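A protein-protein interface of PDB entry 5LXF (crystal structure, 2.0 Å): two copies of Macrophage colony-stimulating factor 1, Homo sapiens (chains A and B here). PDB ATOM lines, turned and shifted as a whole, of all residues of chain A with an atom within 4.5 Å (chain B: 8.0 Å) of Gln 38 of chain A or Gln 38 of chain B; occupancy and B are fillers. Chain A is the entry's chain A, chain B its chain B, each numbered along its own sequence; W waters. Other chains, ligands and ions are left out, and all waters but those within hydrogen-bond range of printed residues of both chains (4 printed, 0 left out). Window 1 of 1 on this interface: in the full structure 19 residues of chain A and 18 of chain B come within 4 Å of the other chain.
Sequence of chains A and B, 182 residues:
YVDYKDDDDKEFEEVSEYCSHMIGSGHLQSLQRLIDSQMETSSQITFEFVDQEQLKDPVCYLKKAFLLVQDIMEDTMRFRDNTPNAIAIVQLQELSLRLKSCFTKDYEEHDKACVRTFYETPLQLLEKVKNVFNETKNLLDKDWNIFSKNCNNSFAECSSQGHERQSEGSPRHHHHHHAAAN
The backbone carbonyl oxygen (O) of Leu 34 of chain A sits at hydrogen-bond distance from the side-chain hydroxyl (OG) of Ser 37 of chain A, at 2.8 Å.
NE2 of Gln 38 of chain A is in hydrogen-bond range of O of Leu 34 of chain A.
The side-chain amide nitrogen (NE2) of Gln 38 of chain A is in hydrogen-bond range of the side-chain hydroxyl (OG) of Ser 37 of chain A.
O of Arg 33 of chain B lies within hydrogen-bond range of OG of Ser 37 of chain B (3.2 Å).
OG of Ser 37 of chain B sits at hydrogen-bond distance from ND2 of Asn 85 of chain B (3.0 Å).
The backbone carbonyl oxygen of Arg 80 of chain B sits at hydrogen-bond distance from the side-chain hydroxyl of Thr 83 of chain B, at 2.8 Å.
The guanidinium group (NH2) of Arg 80 of chain B lies within hydrogen-bond range of the backbone carbonyl oxygen (O) of Ile 35 of chain A (3.2 Å).
OD1 of Asp 36 of chain A lies within salt-bridge range of NE of Arg 80 of chain B (3.0 Å).
The backbone carbonyl oxygen (O) of Ser 37 of chain A lies within hydrogen-bond range of the side-chain amide nitrogen (NE2) of Gln 38 of chain B, 2.8 Å away.
The backbone carbonyl oxygen (O) of Ser 37 of chain A sits at hydrogen-bond distance from the side-chain amide nitrogen (ND2) of Asn 85 of chain B, 2.9 Å away.
The side-chain amide nitrogen of Gln 38 of chain A lies within hydrogen-bond range of the backbone carbonyl oxygen of Ser 37 of chain B.
OE1 of Gln 38 of chain A is in hydrogen-bond range of N of Met 39 of chain B (3.0 Å).
The backbone NH (N) of Met 39 of chain A is in hydrogen-bond range of the side-chain amide oxygen (OE1) of Gln 38 of chain B (2.9 Å).
O of Arg 78 of chain B is in hydrogen-bond range of N of Glu 40 of chain A, 2.8 Å away.
The backbone NH (N) of Arg 80 of chain B sits at hydrogen-bond distance from the side-chain carboxylate (OE2) of Glu 40 of chain A (3.4 Å).
The side-chain amide nitrogen (ND2) of Asn 85 of chain A lies within hydrogen-bond range of the backbone carbonyl oxygen (O) of Ser 37 of chain B, at 2.9 Å.
Water W3 lies within hydrogen-bond range of the backbone carbonyl oxygen (O) of Asp 36 of chain A (2.6 Å) and the backbone NH (N) of Arg 80 of chain B (2.9 Å).
Water W2 bridges the side-chain carboxylate (OE1) of Glu 40 of chain A (2.7 Å) and the backbone carbonyl oxygen (O) of Phe 79 of chain B (2.8 Å).
Water W4 lies within hydrogen-bond range of the backbone carbonyl oxygen (O) of Gln 38 of chain A (2.7 Å), the backbone carbonyl oxygen (O) of Ile 35 of chain A (3.0 Å) and the guanidinium group (NH2) of Arg 80 of chain B (3.3 Å).
Water W1 lies within hydrogen-bond range of the backbone NH (N) of Asn 85 of chain B and the backbone carbonyl oxygen (O) of Asp 36 of chain A.
Ser 37 of chain A touches Gln 38 of chain B, and with the chains exchanged Gln 38 of chain A touches Ser 37 of chain B.
Gln 38 of chain A touches Phe 79 of chain B, and with the chains exchanged Phe 79 of chain A touches Gln 38 of chain B.
Met 39 of chain A touches Leu 34 of chain B, but with the chains exchanged Leu 34 of chain A does not touch Met 39 of chain B (6.2 Å).
Glu 40 of chain A touches Phe 79 of chain B, and with the chains exchanged Phe 79 of chain A touches Glu 40 of chain B.
Of the 26 pairs that touch across the chains among the printed residues, 18 have their exchanged pair printed and touching as well.
Of chain B, only Ser 37 (2.8 Å), Gln 38 (3.7 Å), Met 39 (3.0 Å) and Phe 79 (3.7 Å) come within 4 Å of Gln 38 of chain A.
Gln 38 of chain B touches four residues of chain A.
Ser 37 of chain A touches just these residues of chain B: Ser 37, Gln 38, Phe 79 and Asn 85.
Of the printed residues of chain A, Asn 85 of chain B touches Ser 37 (2.9 Å).
Of the printed residues of chain A, Glu 40 of chain B touches Phe 79.
Ile 35 of chain B touches none of the printed residues of chain A.
Pro 122 of chain B touches none of the printed residues of chain A.
The nearest residue of chain B that does not touch Gln 38 of chain A is Arg 78 of chain B (4.5 Å).
Hydrophobic or aromatic side chains of chain B within 4 Å of the printed part of chain A: Leu 34, Met 39, Met 77, Phe 79 and Leu 126.
Along chain B the printed residues that touch a printed residue of chain A span positions 34 to 126.
Of the 10 printed residues of chain A, 9 touch a printed residue of chain B.
Printed residues of chain A that touch a printed residue of chain B: Ile 35, Asp 36, Ser 37, Gln 38, Met 39, Glu 40, Phe 79, Asn 85 and Leu 126.
Among the printed residues, Asp or Glu carboxylates within 4 Å of a Lys or Arg side-chain nitrogen of the other chain: Asp 36 of chain A with Arg 80 of chain B (2.4 Å).
Among the printed residues, merely in contact across the chains: Met 39 of chain A with Leu 126 of chain B (3.3 Å), Phe 79 of chain A with Ser 37 of chain B (3.4 Å), Met 39 of chain A with Phe 79 of chain B (3.4 Å), Phe 79 of chain A with Met 39 of chain B (3.4 Å), Ser 37 of chain A with Phe 79 of chain B (3.5 Å), Glu 40 of chain A with Phe 79 of chain B (3.5 Å), Ser 37 of chain A with Ser 37 of chain B (3.5 Å), Leu 126 of chain A with Met 39 of chain B (3.6 Å), Met 39 of chain A with Leu 34 of chain B (3.6 Å), Met 39 of chain A with Arg 78 of chain B (3.7 Å), Gln 38 of chain A with Gln 38 of chain B (3.7 Å), Gln 38 of chain A with Phe 79 of chain B (3.7 Å), Met 39 of chain A with Met 77 of chain B (3.8 Å), Phe 79 of chain A with Gln 38 of chain B (3.8 Å), Asp 36 of chain A with Thr 83 of chain B (3.8 Å) and Phe 79 of chain A with Glu 40 of chain B (3.8 Å).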
ATOM      1  N   LEU A  34       9.911 -17.034 -13.234  1.00  0.00           N
ATOM      2  CA  LEU A  34      11.316 -17.430 -13.339  1.00  0.00           C
ATOM      3  C   LEU A  34      11.457 -18.873 -13.818  1.00  0.00           C
ATOM      4  O   LEU A  34      12.177 -19.165 -14.785  1.00  0.00           O
ATOM      5  CB  LEU A  34      12.018 -17.287 -11.986  1.00  0.00           C
ATOM      6  CG  LEU A  34      12.699 -15.984 -11.546  1.00  0.00           C
ATOM      7  CD1 LEU A  34      12.913 -16.007 -10.037  1.00  0.00           C
ATOM      8  CD2 LEU A  34      14.012 -15.780 -12.237  1.00  0.00           C
ATOM      9  N   ILE A  35      10.821 -19.803 -13.092  1.00  0.00           N
ATOM     10  CA  ILE A  35      10.930 -21.214 -13.422  1.00  0.00           C
ATOM     11  C   ILE A  35      10.447 -21.447 -14.838  1.00  0.00           C
ATOM     12  O   ILE A  35      11.090 -22.160 -15.622  1.00  0.00           O
ATOM     13  CB  ILE A  35      10.136 -22.055 -12.405  1.00  0.00           C
ATOM     14  CG1 ILE A  35      10.842 -22.050 -11.041  1.00  0.00           C
ATOM     15  CG2 ILE A  35       9.846 -23.477 -12.953  1.00  0.00           C
ATOM     16  CD1 ILE A  35      10.001 -22.551  -9.902  1.00  0.00           C
ATOM     17  N   ASP A  36       9.328 -20.815 -15.213  1.00  0.00           N
ATOM     18  CA  ASP A  36       8.749 -21.075 -16.540  1.00  0.00           C
ATOM     19  C   ASP A  36       9.604 -20.587 -17.693  1.00  0.00           C
ATOM     20  O   ASP A  36       9.395 -21.055 -18.824  1.00  0.00           O
ATOM     21  CB  ASP A  36       7.327 -20.482 -16.613  1.00  0.00           C
ATOM     22  CG  ASP A  36       6.357 -21.221 -15.703  1.00  0.00           C
ATOM     23  OD1 ASP A  36       6.660 -22.353 -15.303  1.00  0.00           O
ATOM     24  OD2 ASP A  36       5.269 -20.669 -15.388  1.00  0.00           O
ATOM     25  N   SER A  37      10.529 -19.673 -17.447  1.00  0.00           N
ATOM     26  CA  SER A  37      11.342 -19.128 -18.523  1.00  0.00           C
ATOM     27  C   SER A  37      12.646 -19.892 -18.752  1.00  0.00           C
ATOM     28  O   SER A  37      13.354 -19.586 -19.730  1.00  0.00           O
ATOM     29  CB  SER A  37      11.647 -17.638 -18.252  1.00  0.00           C
ATOM     30  OG  SER A  37      12.345 -17.469 -17.022  1.00  0.00           O
ATOM     31  N   GLN A  38      12.978 -20.885 -17.909  1.00  0.00           N
ATOM     32  CA  GLN A  38      14.246 -21.615 -18.033  1.00  0.00           C
ATOM     33  C   GLN A  38      14.136 -22.700 -19.096  1.00  0.00           C
ATOM     34  O   GLN A  38      13.165 -23.463 -19.130  1.00  0.00           O
ATOM     35  CB  GLN A  38      14.654 -22.254 -16.705  1.00  0.00           C
ATOM     36  CG  GLN A  38      14.874 -21.239 -15.599  1.00  0.00           C
ATOM     37  CD  GLN A  38      15.740 -20.069 -16.060  1.00  0.00           C
ATOM     38  OE1 GLN A  38      16.916 -20.246 -16.370  1.00  0.00           O
ATOM     39  NE2 GLN A  38      15.142 -18.887 -16.170  1.00  0.00           N
ATOM     40  N   MET A  39      15.114 -22.722 -19.994  1.00  0.00           N
ATOM     41  CA  MET A  39      15.187 -23.750 -21.025  1.00  0.00           C
ATOM     42  C   MET A  39      15.444 -25.136 -20.430  1.00  0.00           C
ATOM     43  O   MET A  39      16.264 -25.306 -19.525  1.00  0.00           O
ATOM     44  CB  MET A  39      16.227 -23.322 -22.052  1.00  0.00           C
ATOM     45  CG  MET A  39      15.967 -23.840 -23.449  1.00  0.00           C
ATOM     46  SD  MET A  39      17.395 -23.595 -24.512  1.00  0.00           S
ATOM     47  CE  MET A  39      16.884 -22.084 -25.217  1.00  0.00           C
ATOM     48  N   GLU A  40      14.689 -26.126 -20.897  1.00  0.00           N
ATOM     49  CA  GLU A  40      14.865 -27.481 -20.384  1.00  0.00           C
ATOM     50  C   GLU A  40      16.105 -28.077 -21.048  1.00  0.00           C
ATOM     51  O   GLU A  40      16.107 -28.377 -22.243  1.00  0.00           O
ATOM     52  CB  GLU A  40      13.607 -28.298 -20.661  1.00  0.00           C
ATOM     53  CG  GLU A  40      12.353 -27.668 -20.084  1.00  0.00           C
ATOM     54  CD  GLU A  40      11.090 -28.234 -20.700  1.00  0.00           C
ATOM     55  OE1 GLU A  40      11.208 -28.942 -21.726  1.00  0.00           O
ATOM     56  OE2 GLU A  40       9.981 -27.946 -20.184  1.00  0.00           O
ATOM     57  N   PHE A  79      21.098 -13.162 -13.225  1.00  0.00           N
ATOM     58  CA  PHE A  79      20.479 -12.784 -14.483  1.00  0.00           C
ATOM     59  C   PHE A  79      21.038 -11.436 -14.878  1.00  0.00           C
ATOM     60  O   PHE A  79      21.440 -10.646 -14.024  1.00  0.00           O
ATOM     61  CB  PHE A  79      18.950 -12.709 -14.363  1.00  0.00           C
ATOM     62  CG  PHE A  79      18.325 -14.005 -14.002  1.00  0.00           C
ATOM     63  CD1 PHE A  79      18.205 -14.393 -12.678  1.00  0.00           C
ATOM     64  CD2 PHE A  79      17.894 -14.870 -15.002  1.00  0.00           C
ATOM     65  CE1 PHE A  79      17.647 -15.622 -12.351  1.00  0.00           C
ATOM     66  CE2 PHE A  79      17.317 -16.079 -14.690  1.00  0.00           C
ATOM     67  CZ  PHE A  79      17.203 -16.464 -13.360  1.00  0.00           C
ATOM     68  N   ASN A  85      13.751 -11.184 -14.929  1.00  0.00           N
ATOM     69  CA  ASN A  85      14.168 -12.185 -13.955  1.00  0.00           C
ATOM     70  C   ASN A  85      15.173 -11.618 -12.951  1.00  0.00           C
ATOM     71  O   ASN A  85      15.121 -11.955 -11.763  1.00  0.00           O
ATOM     72  CB  ASN A  85      14.728 -13.395 -14.695  1.00  0.00           C
ATOM     73  CG  ASN A  85      13.627 -14.259 -15.294  1.00  0.00           C
ATOM     74  OD1 ASN A  85      12.457 -14.105 -14.953  1.00  0.00           O
ATOM     75  ND2 ASN A  85      13.997 -15.180 -16.156  1.00  0.00           N
ATOM     76  N   LEU A 126      15.759 -23.780  -8.687  1.00  0.00           N
ATOM     77  CA  LEU A 126      14.671 -22.818  -8.615  1.00  0.00           C
ATOM     78  C   LEU A 126      13.455 -23.404  -7.907  1.00  0.00           C
ATOM     79  O   LEU A 126      12.774 -22.702  -7.155  1.00  0.00           O
ATOM     80  CB  LEU A 126      14.322 -22.363 -10.028  1.00  0.00           C
ATOM     81  CG  LEU A 126      15.416 -21.502 -10.656  1.00  0.00           C
ATOM     82  CD1 LEU A 126      15.118 -21.175 -12.107  1.00  0.00           C
ATOM     83  CD2 LEU A 126      15.444 -20.246  -9.900  1.00  0.00           C
ATOM     84  N   LEU B  31      13.899 -13.743 -29.661  1.00  0.00           N
ATOM     85  CA  LEU B  31      15.165 -14.417 -29.403  1.00  0.00           C
ATOM     86  C   LEU B  31      15.907 -13.739 -28.257  1.00  0.00           C
ATOM     87  O   LEU B  31      16.493 -14.410 -27.407  1.00  0.00           O
ATOM     88  CB  LEU B  31      16.023 -14.403 -30.669  1.00  0.00           C
ATOM     89  CG  LEU B  31      15.839 -15.485 -31.736  1.00  0.00           C
ATOM     90  CD1 LEU B  31      16.403 -14.986 -33.055  1.00  0.00           C
ATOM     91  CD2 LEU B  31      16.507 -16.781 -31.364  1.00  0.00           C
ATOM     92  N   GLN B  32      15.893 -12.403 -28.221  1.00  0.00           N
ATOM     93  CA  GLN B  32      16.617 -11.692 -27.172  1.00  0.00           C
ATOM     94  C   GLN B  32      16.006 -11.942 -25.791  1.00  0.00           C
ATOM     95  O   GLN B  32      16.737 -12.155 -24.812  1.00  0.00           O
ATOM     96  CB  GLN B  32      16.660 -10.194 -27.481  1.00  0.00           C
ATOM     97  CG  GLN B  32      17.700  -9.465 -26.637  1.00  0.00           C
ATOM     98  CD  GLN B  32      19.079 -10.116 -26.746  1.00  0.00           C
ATOM     99  OE1 GLN B  32      19.637 -10.245 -27.842  1.00  0.00           O
ATOM    100  NE2 GLN B  32      19.619 -10.557 -25.612  1.00  0.00           N
ATOM    101  N   ARG B  33      14.670 -11.921 -25.692  1.00  0.00           N
ATOM    102  CA  ARG B  33      14.017 -12.214 -24.414  1.00  0.00           C
ATOM    103  C   ARG B  33      14.309 -13.634 -23.973  1.00  0.00           C
ATOM    104  O   ARG B  33      14.550 -13.892 -22.783  1.00  0.00           O
ATOM    105  CB  ARG B  33      12.513 -11.996 -24.525  1.00  0.00           C
ATOM    106  CG  ARG B  33      12.152 -10.535 -24.490  1.00  0.00           C
ATOM    107  CD  ARG B  33      10.659 -10.330 -24.543  1.00  0.00           C
ATOM    108  NE  ARG B  33      10.332  -9.282 -25.499  1.00  0.00           N
ATOM    109  CZ  ARG B  33       9.880  -9.516 -26.725  1.00  0.00           C
ATOM    110  NH1 ARG B  33       9.621  -8.497 -27.531  1.00  0.00           N
ATOM    111  NH2 ARG B  33       9.687 -10.767 -27.147  1.00  0.00           N
ATOM    112  N   LEU B  34      14.297 -14.564 -24.926  1.00  0.00           N
ATOM    113  CA  LEU B  34      14.765 -15.920 -24.694  1.00  0.00           C
ATOM    114  C   LEU B  34      16.120 -15.918 -23.984  1.00  0.00           C
ATOM    115  O   LEU B  34      16.280 -16.498 -22.899  1.00  0.00           O
ATOM    116  CB  LEU B  34      14.857 -16.619 -26.052  1.00  0.00           C
ATOM    117  CG  LEU B  34      14.554 -18.091 -26.198  1.00  0.00           C
ATOM    118  CD1 LEU B  34      15.319 -18.820 -25.127  1.00  0.00           C
ATOM    119  CD2 LEU B  34      13.072 -18.336 -26.096  1.00  0.00           C
ATOM    120  N   ILE B  35      17.109 -15.262 -24.598  1.00  0.00           N
ATOM    121  CA  ILE B  35      18.458 -15.221 -24.039  1.00  0.00           C
ATOM    122  C   ILE B  35      18.463 -14.550 -22.666  1.00  0.00           C
ATOM    123  O   ILE B  35      19.142 -15.012 -21.741  1.00  0.00           O
ATOM    124  CB  ILE B  35      19.419 -14.512 -25.018  1.00  0.00           C
ATOM    125  CG1 ILE B  35      19.667 -15.378 -26.264  1.00  0.00           C
ATOM    126  CG2 ILE B  35      20.736 -14.161 -24.329  1.00  0.00           C
ATOM    127  CD1 ILE B  35      20.389 -14.645 -27.404  1.00  0.00           C
ATOM    128  N   ASP B  36      17.733 -13.433 -22.519  1.00  0.00           N
ATOM    129  CA  ASP B  36      17.815 -12.652 -21.288  1.00  0.00           C
ATOM    130  C   ASP B  36      17.195 -13.358 -20.101  1.00  0.00           C
ATOM    131  O   ASP B  36      17.587 -13.077 -18.967  1.00  0.00           O
ATOM    132  CB  ASP B  36      17.124 -11.290 -21.448  1.00  0.00           C
ATOM    133  CG  ASP B  36      17.847 -10.372 -22.414  1.00  0.00           C
ATOM    134  OD1 ASP B  36      19.016 -10.669 -22.737  1.00  0.00           O
ATOM    135  OD2 ASP B  36      17.256  -9.346 -22.835  1.00  0.00           O
ATOM    136  N   SER B  37      16.278 -14.291 -20.331  1.00  0.00           N
ATOM    137  CA  SER B  37      15.606 -14.943 -19.223  1.00  0.00           C
ATOM    138  C   SER B  37      16.371 -16.147 -18.699  1.00  0.00           C
ATOM    139  O   SER B  37      15.950 -16.723 -17.693  1.00  0.00           O
ATOM    140  CB  SER B  37      14.189 -15.371 -19.629  1.00  0.00           C
ATOM    141  OG  SER B  37      14.214 -16.297 -20.694  1.00  0.00           O
ATOM    142  N   GLN B  38      17.479 -16.537 -19.343  1.00  0.00           N
ATOM    143  CA  GLN B  38      18.205 -17.727 -18.914  1.00  0.00           C
ATOM    144  C   GLN B  38      19.140 -17.387 -17.770  1.00  0.00           C
ATOM    145  O   GLN B  38      19.900 -16.413 -17.838  1.00  0.00           O
ATOM    146  CB  GLN B  38      19.008 -18.336 -20.065  1.00  0.00           C
ATOM    147  CG  GLN B  38      18.143 -18.734 -21.251  1.00  0.00           C
ATOM    148  CD  GLN B  38      16.908 -19.510 -20.820  1.00  0.00           C
ATOM    149  OE1 GLN B  38      17.008 -20.572 -20.195  1.00  0.00           O
ATOM    150  NE2 GLN B  38      15.742 -18.941 -21.077  1.00  0.00           N
ATOM    151  N   MET B  39      19.081 -18.197 -16.719  1.00  0.00           N
ATOM    152  CA  MET B  39      20.055 -18.091 -15.642  1.00  0.00           C
ATOM    153  C   MET B  39      21.463 -18.296 -16.173  1.00  0.00           C
ATOM    154  O   MET B  39      21.718 -19.201 -16.972  1.00  0.00           O
ATOM    155  CB  MET B  39      19.731 -19.102 -14.554  1.00  0.00           C
ATOM    156  CG  MET B  39      20.282 -18.706 -13.205  1.00  0.00           C
ATOM    157  SD  MET B  39      20.250 -20.114 -12.076  1.00  0.00           S
ATOM    158  CE  MET B  39      18.622 -19.872 -11.439  1.00  0.00           C
ATOM    159  N   GLU B  40      22.379 -17.435 -15.747  1.00  0.00           N
ATOM    160  CA  GLU B  40      23.760 -17.527 -16.206  1.00  0.00           C
ATOM    161  C   GLU B  40      24.498 -18.666 -15.512  1.00  0.00           C
ATOM    162  O   GLU B  40      24.458 -18.789 -14.286  1.00  0.00           O
ATOM    163  CB  GLU B  40      24.485 -16.201 -15.987  1.00  0.00           C
ATOM    164  CG  GLU B  40      23.852 -15.046 -16.737  1.00  0.00           C
ATOM    165  CD  GLU B  40      24.270 -13.700 -16.187  1.00  0.00           C
ATOM    166  OE1 GLU B  40      24.071 -12.685 -16.887  1.00  0.00           O
ATOM    167  OE2 GLU B  40      24.812 -13.661 -15.066  1.00  0.00           O
ATOM    168  N   THR B  41      25.093 -19.550 -16.312  1.00  0.00           N
ATOM    169  CA  THR B  41      25.803 -20.708 -15.787  1.00  0.00           C
ATOM    170  C   THR B  41      26.988 -21.021 -16.686  1.00  0.00           C
ATOM    171  O   THR B  41      26.938 -20.812 -17.904  1.00  0.00           O
ATOM    172  CB  THR B  41      24.927 -21.966 -15.709  1.00  0.00           C
ATOM    173  OG1 THR B  41      25.743 -23.069 -15.302  1.00  0.00           O
ATOM    174  CG2 THR B  41      24.309 -22.298 -17.076  1.00  0.00           C
ATOM    175  N   MET B  77      15.885 -26.471 -27.742  1.00  0.00           N
ATOM    176  CA  MET B  77      15.323 -25.239 -27.181  1.00  0.00           C
ATOM    177  C   MET B  77      13.882 -25.489 -26.704  1.00  0.00           C
ATOM    178  O   MET B  77      12.890 -25.022 -27.276  1.00  0.00           O
ATOM    179  CB  MET B  77      15.420 -24.133 -28.225  1.00  0.00           C
ATOM    180  CG  MET B  77      16.894 -23.840 -28.644  1.00  0.00           C
ATOM    181  SD  MET B  77      17.134 -22.403 -29.745  1.00  0.00           S
ATOM    182  CE  MET B  77      17.025 -22.970 -31.361  1.00  0.00           C
ATOM    183  N   ARG B  78      13.778 -26.240 -25.607  1.00  0.00           N
ATOM    184  CA  ARG B  78      12.505 -26.764 -25.121  1.00  0.00           C
ATOM    185  C   ARG B  78      12.024 -26.017 -23.879  1.00  0.00           C
ATOM    186  O   ARG B  78      12.817 -25.731 -22.970  1.00  0.00           O
ATOM    187  CB  ARG B  78      12.638 -28.255 -24.829  1.00  0.00           C
ATOM    188  CG  ARG B  78      13.087 -29.104 -26.060  1.00  0.00           C
ATOM    189  CD  ARG B  78      12.497 -28.577 -27.386  1.00  0.00           C
ATOM    190  NE  ARG B  78      11.033 -28.663 -27.370  1.00  0.00           N
ATOM    191  CZ  ARG B  78      10.219 -28.044 -28.222  1.00  0.00           C
ATOM    192  NH1 ARG B  78      10.701 -27.278 -29.187  1.00  0.00           N
ATOM    193  NH2 ARG B  78       8.910 -28.195 -28.098  1.00  0.00           N
ATOM    194  N   PHE B  79      10.729 -25.682 -23.863  1.00  0.00           N
ATOM    195  CA  PHE B  79      10.082 -25.002 -22.748  1.00  0.00           C
ATOM    196  C   PHE B  79       8.715 -25.640 -22.518  1.00  0.00           C
ATOM    197  O   PHE B  79       8.208 -26.393 -23.352  1.00  0.00           O
ATOM    198  CB  PHE B  79       9.913 -23.504 -23.025  1.00  0.00           C
ATOM    199  CG  PHE B  79      11.213 -22.777 -23.336  1.00  0.00           C
ATOM    200  CD1 PHE B  79      11.714 -22.745 -24.649  1.00  0.00           C
ATOM    201  CD2 PHE B  79      11.932 -22.121 -22.336  1.00  0.00           C
ATOM    202  CE1 PHE B  79      12.899 -22.097 -24.959  1.00  0.00           C
ATOM    203  CE2 PHE B  79      13.127 -21.454 -22.632  1.00  0.00           C
ATOM    204  CZ  PHE B  79      13.617 -21.442 -23.957  1.00  0.00           C
ATOM    205  N   ARG B  80       8.159 -25.376 -21.349  1.00  0.00           N
ATOM    206  CA  ARG B  80       6.765 -25.711 -21.060  1.00  0.00           C
ATOM    207  C   ARG B  80       5.747 -25.123 -22.002  1.00  0.00           C
ATOM    208  O   ARG B  80       5.831 -23.957 -22.388  1.00  0.00           O
ATOM    209  CB  ARG B  80       6.400 -25.210 -19.696  1.00  0.00           C
ATOM    210  CG  ARG B  80       6.926 -25.917 -18.652  1.00  0.00           C
ATOM    211  CD  ARG B  80       5.928 -25.943 -17.592  1.00  0.00           C
ATOM    212  NE  ARG B  80       6.640 -24.802 -17.061  1.00  0.00           N
ATOM    213  CZ  ARG B  80       7.778 -24.915 -16.389  1.00  0.00           C
ATOM    214  NH1 ARG B  80       8.295 -26.070 -16.100  1.00  0.00           N
ATOM    215  NH2 ARG B  80       8.398 -23.865 -15.957  1.00  0.00           N
ATOM    216  N   THR B  83       4.171 -21.317 -22.292  1.00  0.00           N
ATOM    217  CA  THR B  83       4.944 -20.237 -21.675  1.00  0.00           C
ATOM    218  C   THR B  83       5.399 -19.253 -22.754  1.00  0.00           C
ATOM    219  O   THR B  83       5.432 -19.598 -23.938  1.00  0.00           O
ATOM    220  CB  THR B  83       6.155 -20.793 -20.923  1.00  0.00           C
ATOM    221  OG1 THR B  83       7.023 -21.493 -21.836  1.00  0.00           O
ATOM    222  CG2 THR B  83       5.683 -21.738 -19.827  1.00  0.00           C
ATOM    223  N   ASN B  85       8.305 -18.313 -23.660  1.00  0.00           N
ATOM    224  CA  ASN B  85       9.439 -18.792 -24.437  1.00  0.00           C
ATOM    225  C   ASN B  85       9.043 -19.951 -25.352  1.00  0.00           C
ATOM    226  O   ASN B  85       9.559 -20.062 -26.467  1.00  0.00           O
ATOM    227  CB  ASN B  85      10.588 -19.176 -23.503  1.00  0.00           C
ATOM    228  CG  ASN B  85      11.327 -17.967 -22.983  1.00  0.00           C
ATOM    229  OD1 ASN B  85      11.128 -16.854 -23.481  1.00  0.00           O
ATOM    230  ND2 ASN B  85      12.198 -18.169 -21.991  1.00  0.00           N
ATOM    231  N   PRO B 122      24.426 -23.317 -22.630  1.00  0.00           N
ATOM    232  CA  PRO B 122      23.150 -22.943 -23.268  1.00  0.00           C
ATOM    233  C   PRO B 122      23.131 -21.521 -23.798  1.00  0.00           C
ATOM    234  O   PRO B 122      22.541 -21.267 -24.855  1.00  0.00           O
ATOM    235  CB  PRO B 122      22.128 -23.138 -22.134  1.00  0.00           C
ATOM    236  CG  PRO B 122      22.700 -24.245 -21.289  1.00  0.00           C
ATOM    237  CD  PRO B 122      24.224 -24.004 -21.333  1.00  0.00           C
ATOM    238  N   LEU B 123      23.757 -20.578 -23.089  1.00  0.00           N
ATOM    239  CA  LEU B 123      23.773 -19.198 -23.569  1.00  0.00           C
ATOM    240  C   LEU B 123      24.578 -19.076 -24.856  1.00  0.00           C
ATOM    241  O   LEU B 123      24.185 -18.347 -25.777  1.00  0.00           O
ATOM    242  CB  LEU B 123      24.314 -18.256 -22.484  1.00  0.00           C
ATOM    243  CG  LEU B 123      23.260 -17.867 -21.423  1.00  0.00           C
ATOM    244  CD1 LEU B 123      23.814 -16.910 -20.368  1.00  0.00           C
ATOM    245  CD2 LEU B 123      21.979 -17.281 -22.064  1.00  0.00           C
ATOM    246  N   LEU B 126      22.396 -20.381 -27.619  1.00  0.00           N
ATOM    247  CA  LEU B 126      21.369 -19.390 -27.936  1.00  0.00           C
ATOM    248  C   LEU B 126      21.929 -18.224 -28.742  1.00  0.00           C
ATOM    249  O   LEU B 126      21.244 -17.691 -29.627  1.00  0.00           O
ATOM    250  CB  LEU B 126      20.727 -18.883 -26.648  1.00  0.00           C
ATOM    251  CG  LEU B 126      19.822 -19.929 -26.004  1.00  0.00           C
ATOM    252  CD1 LEU B 126      19.244 -19.480 -24.651  1.00  0.00           C
ATOM    253  CD2 LEU B 126      18.751 -20.124 -27.037  1.00  0.00           C
HETATM  254  O   HOH W   1       8.848 -18.382 -20.910  1.00  0.00           O
HETATM  255  O   HOH W   2       9.202 -29.043 -23.526  1.00  0.00           O
HETATM  256  O   HOH W   3       9.639 -23.533 -19.602  1.00  0.00           O
HETATM  257  O   HOH W   4      11.220 -24.452 -17.524  1.00  0.00           O
